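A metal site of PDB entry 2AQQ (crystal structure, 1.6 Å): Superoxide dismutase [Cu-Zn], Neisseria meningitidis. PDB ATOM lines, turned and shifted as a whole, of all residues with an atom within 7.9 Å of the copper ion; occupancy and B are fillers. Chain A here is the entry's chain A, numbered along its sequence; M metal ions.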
ATOM      1  N   GLY A  55      27.295  12.386  -9.414  1.00  0.00           N
ATOM      2  CA  GLY A  55      26.422  11.249  -9.697  1.00  0.00           C
ATOM      3  C   GLY A  55      27.013  10.562 -10.916  1.00  0.00           C
ATOM      4  O   GLY A  55      27.376  11.220 -11.886  1.00  0.00           O
ATOM      5  N   PHE A  56      27.055   9.236 -10.874  1.00  0.00           N
ATOM      6  CA  PHE A  56      27.668   8.438 -11.926  1.00  0.00           C
ATOM      7  C   PHE A  56      26.762   7.220 -12.146  1.00  0.00           C
ATOM      8  O   PHE A  56      26.687   6.344 -11.294  1.00  0.00           O
ATOM      9  CB  PHE A  56      29.044   8.020 -11.388  1.00  0.00           C
ATOM     10  CG  PHE A  56      30.018   7.529 -12.429  1.00  0.00           C
ATOM     11  CD1 PHE A  56      30.109   8.136 -13.686  1.00  0.00           C
ATOM     12  CD2 PHE A  56      30.915   6.516 -12.112  1.00  0.00           C
ATOM     13  CE1 PHE A  56      31.096   7.744 -14.584  1.00  0.00           C
ATOM     14  CE2 PHE A  56      31.906   6.118 -13.003  1.00  0.00           C
ATOM     15  CZ  PHE A  56      31.997   6.740 -14.247  1.00  0.00           C
ATOM     16  N   HIS A  57      26.060   7.190 -13.273  1.00  0.00           N
ATOM     17  CA  HIS A  57      25.148   6.080 -13.553  1.00  0.00           C
ATOM     18  C   HIS A  57      25.083   5.658 -15.016  1.00  0.00           C
ATOM     19  O   HIS A  57      25.421   6.427 -15.914  1.00  0.00           O
ATOM     20  CB  HIS A  57      23.711   6.416 -13.138  1.00  0.00           C
ATOM     21  CG  HIS A  57      23.595   7.475 -12.093  1.00  0.00           C
ATOM     22  ND1 HIS A  57      23.173   8.758 -12.380  1.00  0.00           N
ATOM     23  CD2 HIS A  57      23.820   7.440 -10.760  1.00  0.00           C
ATOM     24  CE1 HIS A  57      23.150   9.469 -11.266  1.00  0.00           C
ATOM     25  NE2 HIS A  57      23.546   8.695 -10.271  1.00  0.00           N
ATOM     26  N   ILE A  58      24.625   4.433 -15.239  1.00  0.00           N
ATOM     27  CA  ILE A  58      24.442   3.937 -16.597  1.00  0.00           C
ATOM     28  C   ILE A  58      23.009   4.356 -16.923  1.00  0.00           C
ATOM     29  O   ILE A  58      22.111   4.113 -16.115  1.00  0.00           O
ATOM     30  CB  ILE A  58      24.485   2.398 -16.678  1.00  0.00           C
ATOM     31  CG1 ILE A  58      25.832   1.877 -16.143  1.00  0.00           C
ATOM     32  CG2 ILE A  58      24.248   1.946 -18.127  1.00  0.00           C
ATOM     33  CD1 ILE A  58      27.037   2.369 -16.917  1.00  0.00           C
ATOM     34  N   HIS A  59      22.800   5.010 -18.065  1.00  0.00           N
ATOM     35  CA  HIS A  59      21.451   5.400 -18.453  1.00  0.00           C
ATOM     36  C   HIS A  59      20.993   4.454 -19.560  1.00  0.00           C
ATOM     37  O   HIS A  59      21.824   3.848 -20.252  1.00  0.00           O
ATOM     38  CB  HIS A  59      21.402   6.861 -18.885  1.00  0.00           C
ATOM     39  CG  HIS A  59      21.385   7.814 -17.728  1.00  0.00           C
ATOM     40  ND1 HIS A  59      20.386   8.753 -17.549  1.00  0.00           N
ATOM     41  CD2 HIS A  59      22.215   7.937 -16.666  1.00  0.00           C
ATOM     42  CE1 HIS A  59      20.606   9.418 -16.428  1.00  0.00           C
ATOM     43  NE2 HIS A  59      21.709   8.943 -15.870  1.00  0.00           N
ATOM     44  N   ALA A  79      19.592  10.317 -23.436  1.00  0.00           N
ATOM     45  CA  ALA A  79      20.076   9.103 -22.795  1.00  0.00           C
ATOM     46  C   ALA A  79      18.976   8.383 -22.012  1.00  0.00           C
ATOM     47  O   ALA A  79      19.109   7.221 -21.650  1.00  0.00           O
ATOM     48  CB  ALA A  79      21.235   9.420 -21.866  1.00  0.00           C
ATOM     49  N   GLY A  80      17.876   9.091 -21.764  1.00  0.00           N
ATOM     50  CA  GLY A  80      16.794   8.484 -21.005  1.00  0.00           C
ATOM     51  C   GLY A  80      17.099   8.479 -19.513  1.00  0.00           C
ATOM     52  O   GLY A  80      17.974   9.216 -19.053  1.00  0.00           O
ATOM     53  N   GLY A  81      16.400   7.637 -18.768  1.00  0.00           N
ATOM     54  CA  GLY A  81      16.612   7.578 -17.331  1.00  0.00           C
ATOM     55  C   GLY A  81      17.684   6.604 -16.918  1.00  0.00           C
ATOM     56  O   GLY A  81      18.418   6.059 -17.749  1.00  0.00           O
ATOM     57  N   HIS A  82      17.797   6.373 -15.613  1.00  0.00           N
ATOM     58  CA  HIS A  82      18.795   5.438 -15.105  1.00  0.00           C
ATOM     59  C   HIS A  82      18.430   4.060 -15.643  1.00  0.00           C
ATOM     60  O   HIS A  82      17.258   3.688 -15.652  1.00  0.00           O
ATOM     61  CB  HIS A  82      18.770   5.406 -13.578  1.00  0.00           C
ATOM     62  CG  HIS A  82      19.230   6.686 -12.935  1.00  0.00           C
ATOM     63  ND1 HIS A  82      19.622   6.746 -11.613  1.00  0.00           N
ATOM     64  CD2 HIS A  82      19.356   7.936 -13.428  1.00  0.00           C
ATOM     65  CE1 HIS A  82      19.951   7.989 -11.312  1.00  0.00           C
ATOM     66  NE2 HIS A  82      19.806   8.733 -12.393  1.00  0.00           N
ATOM     67  N   TRP A  83      19.427   3.309 -16.092  1.00  0.00           N
ATOM     68  CA  TRP A  83      19.163   1.979 -16.615  1.00  0.00           C
ATOM     69  C   TRP A  83      18.552   1.125 -15.501  1.00  0.00           C
ATOM     70  O   TRP A  83      19.159   0.919 -14.448  1.00  0.00           O
ATOM     71  CB  TRP A  83      20.452   1.355 -17.134  1.00  0.00           C
ATOM     72  CG  TRP A  83      20.223   0.091 -17.884  1.00  0.00           C
ATOM     73  CD1 TRP A  83      19.225  -0.147 -18.791  1.00  0.00           C
ATOM     74  CD2 TRP A  83      20.989  -1.111 -17.799  1.00  0.00           C
ATOM     75  NE1 TRP A  83      19.336  -1.437 -19.276  1.00  0.00           N
ATOM     76  CE2 TRP A  83      20.408  -2.037 -18.681  1.00  0.00           C
ATOM     77  CE3 TRP A  83      22.119  -1.483 -17.057  1.00  0.00           C
ATOM     78  CZ2 TRP A  83      20.921  -3.329 -18.856  1.00  0.00           C
ATOM     79  CZ3 TRP A  83      22.633  -2.768 -17.226  1.00  0.00           C
ATOM     80  CH2 TRP A  83      22.031  -3.670 -18.118  1.00  0.00           C
ATOM     81  N   HIS A  91      16.041   4.673  -6.986  1.00  0.00           N
ATOM     82  CA  HIS A  91      17.473   4.959  -7.045  1.00  0.00           C
ATOM     83  C   HIS A  91      18.093   4.539  -5.708  1.00  0.00           C
ATOM     84  O   HIS A  91      17.521   4.806  -4.650  1.00  0.00           O
ATOM     85  CB  HIS A  91      17.722   6.441  -7.293  1.00  0.00           C
ATOM     86  CG  HIS A  91      19.173   6.797  -7.403  1.00  0.00           C
ATOM     87  ND1 HIS A  91      19.955   6.388  -8.463  1.00  0.00           N
ATOM     88  CD2 HIS A  91      19.993   7.463  -6.559  1.00  0.00           C
ATOM     89  CE1 HIS A  91      21.194   6.793  -8.270  1.00  0.00           C
ATOM     90  NE2 HIS A  91      21.251   7.445  -7.124  1.00  0.00           N
ATOM     91  N   GLY A 102      21.719   0.444 -12.999  1.00  0.00           N
ATOM     92  CA  GLY A 102      22.695   1.397 -13.494  1.00  0.00           C
ATOM     93  C   GLY A 102      23.330   2.294 -12.448  1.00  0.00           C
ATOM     94  O   GLY A 102      24.149   3.141 -12.785  1.00  0.00           O
ATOM     95  N   ASP A 103      22.968   2.113 -11.186  1.00  0.00           N
ATOM     96  CA  ASP A 103      23.514   2.958 -10.120  1.00  0.00           C
ATOM     97  C   ASP A 103      24.944   2.574  -9.744  1.00  0.00           C
ATOM     98  O   ASP A 103      25.193   1.525  -9.154  1.00  0.00           O
ATOM     99  CB  ASP A 103      22.599   2.895  -8.883  1.00  0.00           C
ATOM    100  CG  ASP A 103      21.227   3.499  -9.149  1.00  0.00           C
ATOM    101  OD1 ASP A 103      21.088   4.223 -10.163  1.00  0.00           O
ATOM    102  OD2 ASP A 103      20.303   3.271  -8.342  1.00  0.00           O
ATOM    103  N   SER A 134      24.463   4.174 -22.008  1.00  0.00           N
ATOM    104  CA  SER A 134      25.318   5.349 -21.842  1.00  0.00           C
ATOM    105  C   SER A 134      25.770   5.463 -20.402  1.00  0.00           C
ATOM    106  O   SER A 134      25.180   4.877 -19.499  1.00  0.00           O
ATOM    107  CB  SER A 134      24.551   6.608 -22.261  1.00  0.00           C
ATOM    108  OG  SER A 134      23.267   6.649 -21.660  1.00  0.00           O
ATOM    109  N   ILE A 135      26.855   6.202 -20.182  1.00  0.00           N
ATOM    110  CA  ILE A 135      27.351   6.414 -18.825  1.00  0.00           C
ATOM    111  C   ILE A 135      27.259   7.919 -18.628  1.00  0.00           C
ATOM    112  O   ILE A 135      27.727   8.708 -19.450  1.00  0.00           O
ATOM    113  CB  ILE A 135      28.787   5.870 -18.646  1.00  0.00           C
ATOM    114  CG1 ILE A 135      29.214   6.021 -17.186  1.00  0.00           C
ATOM    115  CG2 ILE A 135      29.757   6.570 -19.594  1.00  0.00           C
ATOM    116  CD1 ILE A 135      30.296   5.049 -16.777  1.00  0.00           C
ATOM    117  N   MET A 136      26.633   8.318 -17.535  1.00  0.00           N
ATOM    118  CA  MET A 136      26.390   9.726 -17.250  1.00  0.00           C
ATOM    119  C   MET A 136      27.088  10.260 -16.011  1.00  0.00           C
ATOM    120  O   MET A 136      27.175   9.567 -14.997  1.00  0.00           O
ATOM    121  CB  MET A 136      24.881   9.924 -17.083  1.00  0.00           C
ATOM    122  CG  MET A 136      24.402  11.356 -17.141  1.00  0.00           C
ATOM    123  SD  MET A 136      24.361  11.969 -18.834  1.00  0.00           S
ATOM    124  CE  MET A 136      23.150  10.850 -19.568  1.00  0.00           C
ATOM    125  N   ILE A 137      27.565  11.488 -16.108  1.00  0.00           N
ATOM    126  CA  ILE A 137      28.211  12.162 -14.977  1.00  0.00           C
ATOM    127  C   ILE A 137      27.362  13.403 -14.740  1.00  0.00           C
ATOM    128  O   ILE A 137      27.215  14.243 -15.628  1.00  0.00           O
ATOM    129  CB  ILE A 137      29.654  12.559 -15.297  1.00  0.00           C
ATOM    130  CG1 ILE A 137      30.485  11.305 -15.564  1.00  0.00           C
ATOM    131  CG2 ILE A 137      30.242  13.371 -14.137  1.00  0.00           C
ATOM    132  CD1 ILE A 137      31.891  11.574 -16.084  1.00  0.00           C
ATOM    133  N   HIS A 138      26.791  13.511 -13.549  1.00  0.00           N
ATOM    134  CA  HIS A 138      25.937  14.635 -13.225  1.00  0.00           C
ATOM    135  C   HIS A 138      26.672  15.804 -12.594  1.00  0.00           C
ATOM    136  O   HIS A 138      27.795  15.669 -12.134  1.00  0.00           O
ATOM    137  CB  HIS A 138      24.815  14.158 -12.293  1.00  0.00           C
ATOM    138  CG  HIS A 138      23.862  13.210 -12.948  1.00  0.00           C
ATOM    139  ND1 HIS A 138      22.673  13.619 -13.517  1.00  0.00           N
ATOM    140  CD2 HIS A 138      23.943  11.877 -13.172  1.00  0.00           C
ATOM    141  CE1 HIS A 138      22.057  12.584 -14.049  1.00  0.00           C
ATOM    142  NE2 HIS A 138      22.804  11.509 -13.865  1.00  0.00           N
ATOM    143  N   ASP A 142      25.582  12.273  -5.352  1.00  0.00           N
ATOM    144  CA  ASP A 142      24.711  11.110  -5.274  1.00  0.00           C
ATOM    145  C   ASP A 142      24.615  10.599  -3.837  1.00  0.00           C
ATOM    146  O   ASP A 142      25.598  10.063  -3.294  1.00  0.00           O
ATOM    147  CB  ASP A 142      25.246   9.987  -6.166  1.00  0.00           C
ATOM    148  CG  ASP A 142      24.195   8.935  -6.489  1.00  0.00           C
ATOM    149  OD1 ASP A 142      23.192   8.846  -5.743  1.00  0.00           O
ATOM    150  OD2 ASP A 142      24.354   8.202  -7.481  1.00  0.00           O
ATOM    151  N   LEU A 151      16.658  10.743  -7.619  1.00  0.00           N
ATOM    152  CA  LEU A 151      17.853  10.232  -8.260  1.00  0.00           C
ATOM    153  C   LEU A 151      19.180  10.657  -7.612  1.00  0.00           C
ATOM    154  O   LEU A 151      20.140  10.983  -8.305  1.00  0.00           O
ATOM    155  CB  LEU A 151      17.821  10.637  -9.735  1.00  0.00           C
ATOM    156  CG  LEU A 151      16.493  10.263 -10.410  1.00  0.00           C
ATOM    157  CD1 LEU A 151      16.435  10.830 -11.810  1.00  0.00           C
ATOM    158  CD2 LEU A 151      16.340   8.754 -10.438  1.00  0.00           C
ATOM    159  N   GLY A 154      21.559  14.095  -8.271  1.00  0.00           N
ATOM    160  CA  GLY A 154      22.495  14.311  -9.364  1.00  0.00           C
ATOM    161  C   GLY A 154      22.146  15.551 -10.164  1.00  0.00           C
ATOM    162  O   GLY A 154      23.038  16.256 -10.646  1.00  0.00           O
ATOM    163  N   GLY A 155      20.856  15.812 -10.320  1.00  0.00           N
ATOM    164  CA  GLY A 155      20.443  16.978 -11.077  1.00  0.00           C
ATOM    165  C   GLY A 155      20.845  16.897 -12.544  1.00  0.00           C
ATOM    166  O   GLY A 155      20.831  15.815 -13.134  1.00  0.00           O
ATOM    167  N   PRO A 156      21.198  18.030 -13.159  1.00  0.00           N
ATOM    168  CA  PRO A 156      21.616  18.144 -14.560  1.00  0.00           C
ATOM    169  C   PRO A 156      22.705  17.162 -14.981  1.00  0.00           C
ATOM    170  O   PRO A 156      23.462  16.656 -14.158  1.00  0.00           O
ATOM    171  CB  PRO A 156      22.072  19.593 -14.678  1.00  0.00           C
ATOM    172  CG  PRO A 156      21.185  20.289 -13.707  1.00  0.00           C
ATOM    173  CD  PRO A 156      21.200  19.358 -12.513  1.00  0.00           C
ATOM    174  N   ARG A 157      22.786  16.940 -16.286  1.00  0.00           N
ATOM    175  CA  ARG A 157      23.783  16.027 -16.855  1.00  0.00           C
ATOM    176  C   ARG A 157      24.940  16.859 -17.391  1.00  0.00           C
ATOM    177  O   ARG A 157      24.782  17.645 -18.322  1.00  0.00           O
ATOM    178  CB  ARG A 157      23.108  15.192 -17.939  1.00  0.00           C
ATOM    179  CG  ARG A 157      21.908  14.459 -17.361  1.00  0.00           C
ATOM    180  CD  ARG A 157      21.092  13.683 -18.367  1.00  0.00           C
ATOM    181  NE  ARG A 157      19.920  13.125 -17.703  1.00  0.00           N
ATOM    182  CZ  ARG A 157      19.122  12.197 -18.208  1.00  0.00           C
ATOM    183  NH1 ARG A 157      19.367  11.690 -19.413  1.00  0.00           N
ATOM    184  NH2 ARG A 157      18.087  11.756 -17.502  1.00  0.00           N
ATOM    185  N   ALA A 159      28.400  15.464 -18.105  1.00  0.00           N
ATOM    186  CA  ALA A 159      29.229  14.775 -19.081  1.00  0.00           C
ATOM    187  C   ALA A 159      28.611  13.420 -19.389  1.00  0.00           C
ATOM    188  O   ALA A 159      27.855  12.877 -18.585  1.00  0.00           O
ATOM    189  CB  ALA A 159      30.649  14.609 -18.543  1.00  0.00           C
HETATM  190 CU    CU M   1      22.523   9.504 -14.126  1.00  0.00          CU
HETATM  191 ZN    ZN M   2      19.501   5.314 -10.150  1.00  0.00          ZN
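A ring nitrogen (ND1) of His 59 sits close to the backbone carbonyl oxygen (O) of Gly 81 (3.3 Å).
A ring nitrogen (ND1) of His 59 lies within hydrogen-bond range of the backbone carbonyl oxygen (O) of Gly 80 (2.9 Å).
The backbone NH (N) of His 59 sits at hydrogen-bond distance from the backbone carbonyl oxygen (O) of Ser 134 (2.8 Å).
A ring nitrogen (NE2) of His 82 sits close to a ring nitrogen (ND1) of His 57 (3.4 Å).
O of His 57 lies within hydrogen-bond range of N of Met 136 (2.8 Å).
NE2 of His 57 lies within hydrogen-bond range of OD2 of Asp 142 (2.9 Å).
The backbone NH of His 138 lies within hydrogen-bond range of the backbone carbonyl oxygen of Gly 55 (2.9 Å).
A ring nitrogen (ND1) of His 138 is in hydrogen-bond range of the backbone carbonyl oxygen (O) of Pro 156, at 3.2 Å.
His 82 touches the copper ion (NE2 to CU, 3.3 Å).
Met 136 touches the copper ion (CB to CU, 3.8 Å).
Within 4 Å of the copper ion: His 57, His 59, His 82, Met 136 and His 138.
NE2 of His 59 binds the copper ion (2.0 Å).
The copper ion is bound by ND1 of His 57 (2.0 Å).
The copper ion is bound by a ring nitrogen (NE2) of His 138.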
